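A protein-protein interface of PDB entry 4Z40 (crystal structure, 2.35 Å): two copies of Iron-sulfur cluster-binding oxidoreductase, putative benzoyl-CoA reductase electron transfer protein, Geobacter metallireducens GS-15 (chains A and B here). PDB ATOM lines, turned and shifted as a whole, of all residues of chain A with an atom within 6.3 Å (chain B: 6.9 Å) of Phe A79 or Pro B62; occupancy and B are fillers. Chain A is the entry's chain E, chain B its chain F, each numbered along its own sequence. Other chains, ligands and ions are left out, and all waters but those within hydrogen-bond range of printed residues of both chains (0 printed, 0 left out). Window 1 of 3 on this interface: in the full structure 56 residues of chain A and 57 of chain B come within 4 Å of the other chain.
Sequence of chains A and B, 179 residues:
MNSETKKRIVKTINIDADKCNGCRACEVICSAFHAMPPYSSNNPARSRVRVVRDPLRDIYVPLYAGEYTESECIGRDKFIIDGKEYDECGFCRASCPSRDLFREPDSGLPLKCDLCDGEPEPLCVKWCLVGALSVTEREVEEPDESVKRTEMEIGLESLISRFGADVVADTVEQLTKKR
The backbone carbonyl oxygen (O) of Ile B13 sits at hydrogen-bond distance from the backbone NH (N) of Lys A78 (2.9 Å). N of Ile A80 sits at hydrogen-bond distance from O of Ile B15. N of Ile B15 sits at hydrogen-bond distance from O of Lys A78, 2.9 Å away. The backbone carbonyl oxygen (O) of Ile A80 is in hydrogen-bond range of the backbone NH (N) of Ala B17, 3.2 Å away.
N of Tyr A86 lies within hydrogen-bond range of O of Phe A79. NE of Arg B93 lies within hydrogen-bond range of O of Tyr B64 (2.9 Å). The backbone NH (N) of Val B52 is in hydrogen-bond range of the backbone carbonyl oxygen (O) of Val B61 (2.5 Å). The backbone carbonyl oxygen (O) of Ala B132 sits at hydrogen-bond distance from the backbone NH (N) of Asp B16, 3.0 Å away.
Among the printed residues, merely in contact across the chains: Asp A77 with Ile B13, Asp A77 with Arg B93, Lys A78 with Asn B14, Phe A79 with Ile B15, Phe A79 with Val B61, Phe A79 with Pro B62, Ile A80 with Asp B16, Ile A81 with Phe B91 and Phe A91 with Phe B91.
Printed residues of chain B within 4 Å of Phe A79: Ile B15, Val B61 and Pro B62. Lys A84 touches none of the printed residues of chain B. Of the printed residues of chain A, Ile B13 touches Asp A77 (3.6 Å) and Lys A78 (2.9 Å). Cys B20 touches none of the printed residues of chain A. Printed residues of chain A within 4 Å of Val B61: Phe A79. Pro B62 touches just one residue of chain A: Phe A79 (3.5 Å). Of the printed residues of chain A, Phe B91 touches Ile A81 and Phe A91. Of the printed residues of chain A, Arg B93 touches Asp A77.
Of the 22 printed residues of chain B, 9 touch a printed residue of chain A. Among the printed residues, no Asp or Glu carboxylate lies within 4 Å of a Lys or Arg side-chain nitrogen of the other chain.
Phe A91 touches its own counterpart, Phe B91.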
ATOM      1  N   ASP A  77       8.328 -27.761 -20.240  1.00  0.00           N
ATOM      2  CA  ASP A  77       9.172 -27.456 -19.079  1.00  0.00           C
ATOM      3  C   ASP A  77       9.051 -28.492 -17.943  1.00  0.00           C
ATOM      4  O   ASP A  77       7.983 -29.048 -17.690  1.00  0.00           O
ATOM      5  CB  ASP A  77       8.877 -26.040 -18.553  1.00  0.00           C
ATOM      6  CG  ASP A  77       7.508 -25.917 -17.847  1.00  0.00           C
ATOM      7  OD1 ASP A  77       6.592 -26.731 -18.104  1.00  0.00           O
ATOM      8  OD2 ASP A  77       7.347 -24.957 -17.046  1.00  0.00           O
ATOM      9  N   LYS A  78      10.175 -28.749 -17.278  1.00  0.00           N
ATOM     10  CA  LYS A  78      10.286 -29.800 -16.277  1.00  0.00           C
ATOM     11  C   LYS A  78      11.088 -29.283 -15.094  1.00  0.00           C
ATOM     12  O   LYS A  78      12.285 -29.010 -15.211  1.00  0.00           O
ATOM     13  CB  LYS A  78      10.948 -31.040 -16.876  1.00  0.00           C
ATOM     14  CG  LYS A  78      10.696 -32.362 -16.116  1.00  0.00           C
ATOM     15  CD  LYS A  78      11.223 -33.537 -16.923  1.00  0.00           C
ATOM     16  CE  LYS A  78      10.801 -34.881 -16.347  1.00  0.00           C
ATOM     17  NZ  LYS A  78      11.395 -35.066 -14.999  1.00  0.00           N
ATOM     18  N   PHE A  79      10.430 -29.127 -13.953  1.00  0.00           N
ATOM     19  CA  PHE A  79      11.090 -28.534 -12.794  1.00  0.00           C
ATOM     20  C   PHE A  79      11.692 -29.559 -11.834  1.00  0.00           C
ATOM     21  O   PHE A  79      11.180 -30.659 -11.680  1.00  0.00           O
ATOM     22  CB  PHE A  79      10.115 -27.661 -12.012  1.00  0.00           C
ATOM     23  CG  PHE A  79       9.770 -26.378 -12.685  1.00  0.00           C
ATOM     24  CD1 PHE A  79      10.690 -25.337 -12.735  1.00  0.00           C
ATOM     25  CD2 PHE A  79       8.520 -26.194 -13.255  1.00  0.00           C
ATOM     26  CE1 PHE A  79      10.374 -24.144 -13.351  1.00  0.00           C
ATOM     27  CE2 PHE A  79       8.201 -24.999 -13.877  1.00  0.00           C
ATOM     28  CZ  PHE A  79       9.126 -23.975 -13.916  1.00  0.00           C
ATOM     29  N   ILE A  80      12.791 -29.170 -11.203  1.00  0.00           N
ATOM     30  CA  ILE A  80      13.254 -29.793  -9.979  1.00  0.00           C
ATOM     31  C   ILE A  80      13.265 -28.732  -8.889  1.00  0.00           C
ATOM     32  O   ILE A  80      14.026 -27.768  -8.966  1.00  0.00           O
ATOM     33  CB  ILE A  80      14.648 -30.399 -10.122  1.00  0.00           C
ATOM     34  CG1 ILE A  80      14.605 -31.599 -11.069  1.00  0.00           C
ATOM     35  CG2 ILE A  80      15.176 -30.814  -8.752  1.00  0.00           C
ATOM     36  CD1 ILE A  80      15.968 -32.172 -11.363  1.00  0.00           C
ATOM     37  N   ILE A  81      12.406 -28.897  -7.889  1.00  0.00           N
ATOM     38  CA  ILE A  81      12.293 -27.899  -6.832  1.00  0.00           C
ATOM     39  C   ILE A  81      12.391 -28.500  -5.436  1.00  0.00           C
ATOM     40  O   ILE A  81      11.577 -29.351  -5.060  1.00  0.00           O
ATOM     41  CB  ILE A  81      10.966 -27.125  -6.920  1.00  0.00           C
ATOM     42  CG1 ILE A  81      10.695 -26.676  -8.356  1.00  0.00           C
ATOM     43  CG2 ILE A  81      10.978 -25.942  -5.946  1.00  0.00           C
ATOM     44  CD1 ILE A  81       9.392 -25.929  -8.521  1.00  0.00           C
ATOM     45  N   LYS A  84      12.421 -32.280  -5.240  1.00  0.00           N
ATOM     46  CA  LYS A  84      11.370 -33.052  -5.903  1.00  0.00           C
ATOM     47  C   LYS A  84      11.419 -32.905  -7.413  1.00  0.00           C
ATOM     48  O   LYS A  84      11.515 -31.804  -7.936  1.00  0.00           O
ATOM     49  CB  LYS A  84       9.994 -32.628  -5.391  1.00  0.00           C
ATOM     50  CG  LYS A  84       9.792 -32.862  -3.917  1.00  0.00           C
ATOM     51  CD  LYS A  84       8.432 -32.376  -3.460  1.00  0.00           C
ATOM     52  CE  LYS A  84       8.028 -33.081  -2.167  1.00  0.00           C
ATOM     53  NZ  LYS A  84       6.781 -32.514  -1.595  1.00  0.00           N
ATOM     54  N   GLU A  85      11.339 -34.026  -8.117  1.00  0.00           N
ATOM     55  CA  GLU A  85      11.388 -34.008  -9.570  1.00  0.00           C
ATOM     56  C   GLU A  85       9.988 -34.065 -10.154  1.00  0.00           C
ATOM     57  O   GLU A  85       9.431 -35.142 -10.326  1.00  0.00           O
ATOM     58  CB  GLU A  85      12.242 -35.162 -10.074  1.00  0.00           C
ATOM     59  CG  GLU A  85      13.564 -35.265  -9.328  1.00  0.00           C
ATOM     60  CD  GLU A  85      14.614 -36.080 -10.068  1.00  0.00           C
ATOM     61  OE1 GLU A  85      14.330 -37.237 -10.434  1.00  0.00           O
ATOM     62  OE2 GLU A  85      15.734 -35.554 -10.284  1.00  0.00           O
ATOM     63  N   TYR A  86       9.423 -32.899 -10.466  1.00  0.00           N
ATOM     64  CA  TYR A  86       8.038 -32.814 -10.919  1.00  0.00           C
ATOM     65  C   TYR A  86       7.896 -33.300 -12.355  1.00  0.00           C
ATOM     66  O   TYR A  86       8.890 -33.553 -13.038  1.00  0.00           O
ATOM     67  CB  TYR A  86       7.513 -31.385 -10.783  1.00  0.00           C
ATOM     68  CG  TYR A  86       7.390 -30.903  -9.346  1.00  0.00           C
ATOM     69  CD1 TYR A  86       8.470 -30.317  -8.685  1.00  0.00           C
ATOM     70  CD2 TYR A  86       6.194 -31.046  -8.648  1.00  0.00           C
ATOM     71  CE1 TYR A  86       8.359 -29.895  -7.369  1.00  0.00           C
ATOM     72  CE2 TYR A  86       6.073 -30.627  -7.333  1.00  0.00           C
ATOM     73  CZ  TYR A  86       7.155 -30.051  -6.696  1.00  0.00           C
ATOM     74  OH  TYR A  86       7.023 -29.629  -5.381  1.00  0.00           O
ATOM     75  N   ASP A  87       6.653 -33.449 -12.803  1.00  0.00           N
ATOM     76  CA  ASP A  87       6.392 -33.927 -14.156  1.00  0.00           C
ATOM     77  C   ASP A  87       6.526 -32.795 -15.173  1.00  0.00           C
ATOM     78  O   ASP A  87       6.362 -31.628 -14.844  1.00  0.00           O
ATOM     79  CB  ASP A  87       4.996 -34.552 -14.246  1.00  0.00           C
ATOM     80  CG  ASP A  87       4.899 -35.883 -13.503  1.00  0.00           C
ATOM     81  OD1 ASP A  87       5.732 -36.787 -13.764  1.00  0.00           O
ATOM     82  OD2 ASP A  87       3.994 -36.027 -12.648  1.00  0.00           O
ATOM     83  N   GLU A  88       6.853 -33.166 -16.403  1.00  0.00           N
ATOM     84  CA  GLU A  88       6.783 -32.290 -17.562  1.00  0.00           C
ATOM     85  C   GLU A  88       5.432 -31.575 -17.661  1.00  0.00           C
ATOM     86  O   GLU A  88       4.411 -32.226 -17.712  1.00  0.00           O
ATOM     87  CB  GLU A  88       7.031 -33.132 -18.810  1.00  0.00           C
ATOM     88  CG  GLU A  88       7.149 -32.393 -20.131  1.00  0.00           C
ATOM     89  CD  GLU A  88       7.233 -33.382 -21.277  1.00  0.00           C
ATOM     90  OE1 GLU A  88       6.243 -34.123 -21.498  1.00  0.00           O
ATOM     91  OE2 GLU A  88       8.296 -33.439 -21.933  1.00  0.00           O
ATOM     92  N   GLY A  90       4.152 -29.972 -15.302  1.00  0.00           N
ATOM     93  CA  GLY A  90       3.594 -30.301 -14.006  1.00  0.00           C
ATOM     94  C   GLY A  90       2.606 -29.301 -13.446  1.00  0.00           C
ATOM     95  O   GLY A  90       1.614 -29.689 -12.838  1.00  0.00           O
ATOM     96  N   PHE A  91       2.869 -28.019 -13.658  1.00  0.00           N
ATOM     97  CA  PHE A  91       2.061 -26.946 -13.078  1.00  0.00           C
ATOM     98  C   PHE A  91       1.233 -26.168 -14.102  1.00  0.00           C
ATOM     99  O   PHE A  91       0.654 -25.148 -13.774  1.00  0.00           O
ATOM    100  CB  PHE A  91       2.959 -25.965 -12.323  1.00  0.00           C
ATOM    101  CG  PHE A  91       3.783 -26.607 -11.242  1.00  0.00           C
ATOM    102  CD1 PHE A  91       3.323 -26.656  -9.943  1.00  0.00           C
ATOM    103  CD2 PHE A  91       5.017 -27.166 -11.532  1.00  0.00           C
ATOM    104  CE1 PHE A  91       4.078 -27.244  -8.956  1.00  0.00           C
ATOM    105  CE2 PHE A  91       5.781 -27.755 -10.543  1.00  0.00           C
ATOM    106  CZ  PHE A  91       5.308 -27.797  -9.258  1.00  0.00           C
ATOM    107  N   ILE B  13      12.527 -28.583 -21.607  1.00  0.00           N
ATOM    108  CA  ILE B  13      13.446 -27.693 -20.898  1.00  0.00           C
ATOM    109  C   ILE B  13      13.598 -28.113 -19.427  1.00  0.00           C
ATOM    110  O   ILE B  13      12.665 -28.000 -18.628  1.00  0.00           O
ATOM    111  CB  ILE B  13      12.975 -26.242 -20.958  1.00  0.00           C
ATOM    112  CG1 ILE B  13      12.601 -25.873 -22.394  1.00  0.00           C
ATOM    113  CG2 ILE B  13      14.072 -25.312 -20.462  1.00  0.00           C
ATOM    114  CD1 ILE B  13      11.907 -24.563 -22.514  1.00  0.00           C
ATOM    115  N   ASN B  14      14.781 -28.598 -19.078  1.00  0.00           N
ATOM    116  CA  ASN B  14      15.031 -29.083 -17.735  1.00  0.00           C
ATOM    117  C   ASN B  14      15.537 -27.972 -16.844  1.00  0.00           C
ATOM    118  O   ASN B  14      16.673 -27.508 -16.976  1.00  0.00           O
ATOM    119  CB  ASN B  14      16.022 -30.237 -17.777  1.00  0.00           C
ATOM    120  CG  ASN B  14      15.629 -31.275 -18.794  1.00  0.00           C
ATOM    121  OD1 ASN B  14      14.519 -31.792 -18.757  1.00  0.00           O
ATOM    122  ND2 ASN B  14      16.517 -31.555 -19.739  1.00  0.00           N
ATOM    123  N   ILE B  15      14.679 -27.547 -15.931  1.00  0.00           N
ATOM    124  CA  ILE B  15      15.007 -26.479 -15.008  1.00  0.00           C
ATOM    125  C   ILE B  15      15.264 -26.994 -13.585  1.00  0.00           C
ATOM    126  O   ILE B  15      14.324 -27.277 -12.842  1.00  0.00           O
ATOM    127  CB  ILE B  15      13.872 -25.451 -14.957  1.00  0.00           C
ATOM    128  CG1 ILE B  15      13.403 -25.113 -16.375  1.00  0.00           C
ATOM    129  CG2 ILE B  15      14.296 -24.254 -14.157  1.00  0.00           C
ATOM    130  CD1 ILE B  15      12.208 -24.154 -16.443  1.00  0.00           C
ATOM    131  N   ASP B  16      16.540 -27.106 -13.224  1.00  0.00           N
ATOM    132  CA  ASP B  16      16.955 -27.394 -11.855  1.00  0.00           C
ATOM    133  C   ASP B  16      17.030 -26.112 -11.016  1.00  0.00           C
ATOM    134  O   ASP B  16      18.098 -25.513 -10.876  1.00  0.00           O
ATOM    135  CB  ASP B  16      18.314 -28.091 -11.855  1.00  0.00           C
ATOM    136  CG  ASP B  16      18.622 -28.786 -10.540  1.00  0.00           C
ATOM    137  OD1 ASP B  16      18.086 -28.367  -9.488  1.00  0.00           O
ATOM    138  OD2 ASP B  16      19.404 -29.763 -10.564  1.00  0.00           O
ATOM    139  N   ALA B  17      15.904 -25.706 -10.439  1.00  0.00           N
ATOM    140  CA  ALA B  17      15.830 -24.454  -9.690  1.00  0.00           C
ATOM    141  C   ALA B  17      16.515 -24.537  -8.324  1.00  0.00           C
ATOM    142  O   ALA B  17      16.553 -23.550  -7.580  1.00  0.00           O
ATOM    143  CB  ALA B  17      14.382 -24.034  -9.526  1.00  0.00           C
ATOM    144  N   CYS B  20      19.865 -22.817  -9.339  1.00  0.00           N
ATOM    145  CA  CYS B  20      19.811 -21.422  -9.745  1.00  0.00           C
ATOM    146  C   CYS B  20      20.378 -20.513  -8.663  1.00  0.00           C
ATOM    147  O   CYS B  20      20.166 -20.737  -7.467  1.00  0.00           O
ATOM    148  CB  CYS B  20      18.377 -21.015 -10.076  1.00  0.00           C
ATOM    149  SG  CYS B  20      18.217 -19.351 -10.791  1.00  0.00           S
ATOM    150  N   CYS B  26      20.409 -15.347 -17.892  1.00  0.00           N
ATOM    151  CA  CYS B  26      19.450 -15.849 -18.863  1.00  0.00           C
ATOM    152  C   CYS B  26      18.516 -14.757 -19.362  1.00  0.00           C
ATOM    153  O   CYS B  26      18.053 -14.816 -20.485  1.00  0.00           O
ATOM    154  CB  CYS B  26      18.631 -17.003 -18.255  1.00  0.00           C
ATOM    155  SG  CYS B  26      17.952 -16.697 -16.577  1.00  0.00           S
ATOM    156  N   VAL B  49      12.522 -15.733 -21.086  1.00  0.00           N
ATOM    157  CA  VAL B  49      12.684 -16.449 -19.830  1.00  0.00           C
ATOM    158  C   VAL B  49      12.779 -15.427 -18.691  1.00  0.00           C
ATOM    159  O   VAL B  49      13.527 -14.432 -18.778  1.00  0.00           O
ATOM    160  CB  VAL B  49      13.926 -17.354 -19.828  1.00  0.00           C
ATOM    161  CG1 VAL B  49      15.138 -16.611 -20.358  1.00  0.00           C
ATOM    162  CG2 VAL B  49      14.186 -17.890 -18.412  1.00  0.00           C
ATOM    163  N   ARG B  50      11.995 -15.644 -17.637  1.00  0.00           N
ATOM    164  CA  ARG B  50      11.931 -14.670 -16.561  1.00  0.00           C
ATOM    165  C   ARG B  50      12.003 -15.363 -15.205  1.00  0.00           C
ATOM    166  O   ARG B  50      11.146 -16.189 -14.869  1.00  0.00           O
ATOM    167  CB  ARG B  50      10.656 -13.825 -16.672  1.00  0.00           C
ATOM    168  CG  ARG B  50      10.474 -13.105 -18.008  1.00  0.00           C
ATOM    169  CD  ARG B  50      11.484 -11.953 -18.199  1.00  0.00           C
ATOM    170  NE  ARG B  50      11.579 -11.089 -17.025  1.00  0.00           N
ATOM    171  CZ  ARG B  50      10.714 -10.126 -16.718  1.00  0.00           C
ATOM    172  NH1 ARG B  50       9.672  -9.889 -17.500  1.00  0.00           N
ATOM    173  NH2 ARG B  50      10.889  -9.400 -15.621  1.00  0.00           N
ATOM    174  N   VAL B  51      13.026 -15.015 -14.430  1.00  0.00           N
ATOM    175  CA  VAL B  51      13.294 -15.682 -13.164  1.00  0.00           C
ATOM    176  C   VAL B  51      12.411 -15.148 -12.044  1.00  0.00           C
ATOM    177  O   VAL B  51      12.362 -13.951 -11.821  1.00  0.00           O
ATOM    178  CB  VAL B  51      14.780 -15.526 -12.756  1.00  0.00           C
ATOM    179  CG1 VAL B  51      15.027 -16.120 -11.388  1.00  0.00           C
ATOM    180  CG2 VAL B  51      15.711 -16.152 -13.807  1.00  0.00           C
ATOM    181  N   VAL B  52      11.696 -16.035 -11.354  1.00  0.00           N
ATOM    182  CA  VAL B  52      11.030 -15.633 -10.125  1.00  0.00           C
ATOM    183  C   VAL B  52      12.079 -15.698  -9.008  1.00  0.00           C
ATOM    184  O   VAL B  52      12.669 -16.755  -8.779  1.00  0.00           O
ATOM    185  CB  VAL B  52       9.813 -16.530  -9.777  1.00  0.00           C
ATOM    186  CG1 VAL B  52       9.200 -16.064  -8.470  1.00  0.00           C
ATOM    187  CG2 VAL B  52       8.768 -16.503 -10.889  1.00  0.00           C
ATOM    188  N   TYR B  60      13.936 -19.238  -6.225  1.00  0.00           N
ATOM    189  CA  TYR B  60      14.573 -18.944  -7.494  1.00  0.00           C
ATOM    190  C   TYR B  60      14.001 -19.866  -8.561  1.00  0.00           C
ATOM    191  O   TYR B  60      14.482 -20.987  -8.740  1.00  0.00           O
ATOM    192  CB  TYR B  60      16.088 -19.126  -7.395  1.00  0.00           C
ATOM    193  CG  TYR B  60      16.733 -18.381  -6.247  1.00  0.00           C
ATOM    194  CD1 TYR B  60      17.204 -17.089  -6.420  1.00  0.00           C
ATOM    195  CD2 TYR B  60      16.875 -18.971  -4.988  1.00  0.00           C
ATOM    196  CE1 TYR B  60      17.799 -16.393  -5.384  1.00  0.00           C
ATOM    197  CE2 TYR B  60      17.475 -18.283  -3.939  1.00  0.00           C
ATOM    198  CZ  TYR B  60      17.936 -16.987  -4.146  1.00  0.00           C
ATOM    199  OH  TYR B  60      18.536 -16.270  -3.130  1.00  0.00           O
ATOM    200  N   VAL B  61      12.969 -19.408  -9.265  1.00  0.00           N
ATOM    201  CA  VAL B  61      12.385 -20.210 -10.341  1.00  0.00           C
ATOM    202  C   VAL B  61      12.442 -19.516 -11.715  1.00  0.00           C
ATOM    203  O   VAL B  61      11.817 -18.473 -11.920  1.00  0.00           O
ATOM    204  CB  VAL B  61      10.917 -20.563 -10.044  1.00  0.00           C
ATOM    205  CG1 VAL B  61      10.552 -21.827 -10.752  1.00  0.00           C
ATOM    206  CG2 VAL B  61      10.683 -20.684  -8.555  1.00  0.00           C
ATOM    207  N   PRO B  62      13.203 -20.092 -12.659  1.00  0.00           N
ATOM    208  CA  PRO B  62      13.201 -19.616 -14.052  1.00  0.00           C
ATOM    209  C   PRO B  62      11.943 -20.061 -14.793  1.00  0.00           C
ATOM    210  O   PRO B  62      11.610 -21.240 -14.791  1.00  0.00           O
ATOM    211  CB  PRO B  62      14.445 -20.273 -14.658  1.00  0.00           C
ATOM    212  CG  PRO B  62      15.273 -20.701 -13.498  1.00  0.00           C
ATOM    213  CD  PRO B  62      14.294 -21.046 -12.408  1.00  0.00           C
ATOM    214  N   LEU B  63      11.259 -19.121 -15.425  1.00  0.00           N
ATOM    215  CA  LEU B  63       9.986 -19.391 -16.081  1.00  0.00           C
ATOM    216  C   LEU B  63      10.019 -19.018 -17.570  1.00  0.00           C
ATOM    217  O   LEU B  63      10.338 -17.880 -17.923  1.00  0.00           O
ATOM    218  CB  LEU B  63       8.885 -18.613 -15.372  1.00  0.00           C
ATOM    219  CG  LEU B  63       7.591 -19.283 -14.944  1.00  0.00           C
ATOM    220  CD1 LEU B  63       6.586 -18.195 -14.618  1.00  0.00           C
ATOM    221  CD2 LEU B  63       7.055 -20.205 -16.014  1.00  0.00           C
ATOM    222  N   TYR B  64       9.681 -19.970 -18.437  1.00  0.00           N
ATOM    223  CA  TYR B  64       9.726 -19.772 -19.889  1.00  0.00           C
ATOM    224  C   TYR B  64       8.380 -19.384 -20.478  1.00  0.00           C
ATOM    225  O   TYR B  64       7.369 -20.009 -20.180  1.00  0.00           O
ATOM    226  CB  TYR B  64      10.223 -21.037 -20.584  1.00  0.00           C
ATOM    227  CG  TYR B  64      11.697 -21.248 -20.421  1.00  0.00           C
ATOM    228  CD1 TYR B  64      12.219 -21.636 -19.199  1.00  0.00           C
ATOM    229  CD2 TYR B  64      12.577 -21.036 -21.487  1.00  0.00           C
ATOM    230  CE1 TYR B  64      13.568 -21.823 -19.029  1.00  0.00           C
ATOM    231  CE2 TYR B  64      13.946 -21.213 -21.326  1.00  0.00           C
ATOM    232  CZ  TYR B  64      14.428 -21.612 -20.089  1.00  0.00           C
ATOM    233  OH  TYR B  64      15.774 -21.804 -19.896  1.00  0.00           O
ATOM    234  N   GLY B  90       2.241 -17.934 -10.158  1.00  0.00           N
ATOM    235  CA  GLY B  90       3.689 -18.034 -10.132  1.00  0.00           C
ATOM    236  C   GLY B  90       4.349 -19.156 -10.913  1.00  0.00           C
ATOM    237  O   GLY B  90       5.569 -19.241 -10.929  1.00  0.00           O
ATOM    238  N   PHE B  91       3.565 -20.028 -11.539  1.00  0.00           N
ATOM    239  CA  PHE B  91       4.127 -21.086 -12.387  1.00  0.00           C
ATOM    240  C   PHE B  91       3.558 -21.035 -13.808  1.00  0.00           C
ATOM    241  O   PHE B  91       3.911 -21.843 -14.667  1.00  0.00           O
ATOM    242  CB  PHE B  91       3.868 -22.463 -11.774  1.00  0.00           C
ATOM    243  CG  PHE B  91       4.700 -22.748 -10.556  1.00  0.00           C
ATOM    244  CD1 PHE B  91       6.046 -23.061 -10.677  1.00  0.00           C
ATOM    245  CD2 PHE B  91       4.144 -22.693  -9.293  1.00  0.00           C
ATOM    246  CE1 PHE B  91       6.819 -23.321  -9.551  1.00  0.00           C
ATOM    247  CE2 PHE B  91       4.912 -22.941  -8.167  1.00  0.00           C
ATOM    248  CZ  PHE B  91       6.250 -23.259  -8.296  1.00  0.00           C
ATOM    249  N   ARG B  93       2.997 -20.199 -17.546  1.00  0.00           N
ATOM    250  CA  ARG B  93       3.836 -19.760 -18.656  1.00  0.00           C
ATOM    251  C   ARG B  93       3.095 -18.840 -19.631  1.00  0.00           C
ATOM    252  O   ARG B  93       3.689 -18.312 -20.576  1.00  0.00           O
ATOM    253  CB  ARG B  93       4.377 -20.957 -19.434  1.00  0.00           C
ATOM    254  CG  ARG B  93       5.225 -21.914 -18.619  1.00  0.00           C
ATOM    255  CD  ARG B  93       5.642 -23.094 -19.461  1.00  0.00           C
ATOM    256  NE  ARG B  93       6.392 -22.663 -20.640  1.00  0.00           N
ATOM    257  CZ  ARG B  93       6.755 -23.470 -21.640  1.00  0.00           C
ATOM    258  NH1 ARG B  93       6.417 -24.766 -21.624  1.00  0.00           N
ATOM    259  NH2 ARG B  93       7.443 -22.976 -22.666  1.00  0.00           N
ATOM    260  N   PHE B 102       6.190 -11.881 -20.043  1.00  0.00           N
ATOM    261  CA  PHE B 102       6.008 -12.469 -21.363  1.00  0.00           C
ATOM    262  C   PHE B 102       5.148 -11.586 -22.271  1.00  0.00           C
ATOM    263  O   PHE B 102       4.490 -12.069 -23.193  1.00  0.00           O
ATOM    264  CB  PHE B 102       5.395 -13.866 -21.220  1.00  0.00           C
ATOM    265  CG  PHE B 102       6.123 -14.753 -20.245  1.00  0.00           C
ATOM    266  CD1 PHE B 102       7.509 -14.827 -20.247  1.00  0.00           C
ATOM    267  CD2 PHE B 102       5.424 -15.499 -19.311  1.00  0.00           C
ATOM    268  CE1 PHE B 102       8.186 -15.650 -19.351  1.00  0.00           C
ATOM    269  CE2 PHE B 102       6.095 -16.320 -18.411  1.00  0.00           C
ATOM    270  CZ  PHE B 102       7.479 -16.389 -18.429  1.00  0.00           C
ATOM    271  N   ALA B 132      22.163 -24.724 -14.452  1.00  0.00           N
ATOM    272  CA  ALA B 132      20.819 -24.928 -13.934  1.00  0.00           C
ATOM    273  C   ALA B 132      19.849 -25.299 -15.057  1.00  0.00           C
ATOM    274  O   ALA B 132      18.832 -25.945 -14.803  1.00  0.00           O
ATOM    275  CB  ALA B 132      20.332 -23.678 -13.217  1.00  0.00           C
ATOM    276  N   LEU B 133      20.153 -24.880 -16.289  1.00  0.00           N
ATOM    277  CA  LEU B 133      19.246 -25.115 -17.412  1.00  0.00           C
ATOM    278  C   LEU B 133      19.808 -26.092 -18.427  1.00  0.00           C
ATOM    279  O   LEU B 133      21.015 -26.194 -18.600  1.00  0.00           O
ATOM    280  CB  LEU B 133      18.923 -23.812 -18.125  1.00  0.00           C
ATOM    281  CG  LEU B 133      18.403 -22.623 -17.324  1.00  0.00           C
ATOM    282  CD1 LEU B 133      18.361 -21.360 -18.219  1.00  0.00           C
ATOM    283  CD2 LEU B 133      17.037 -22.938 -16.715  1.00  0.00           C
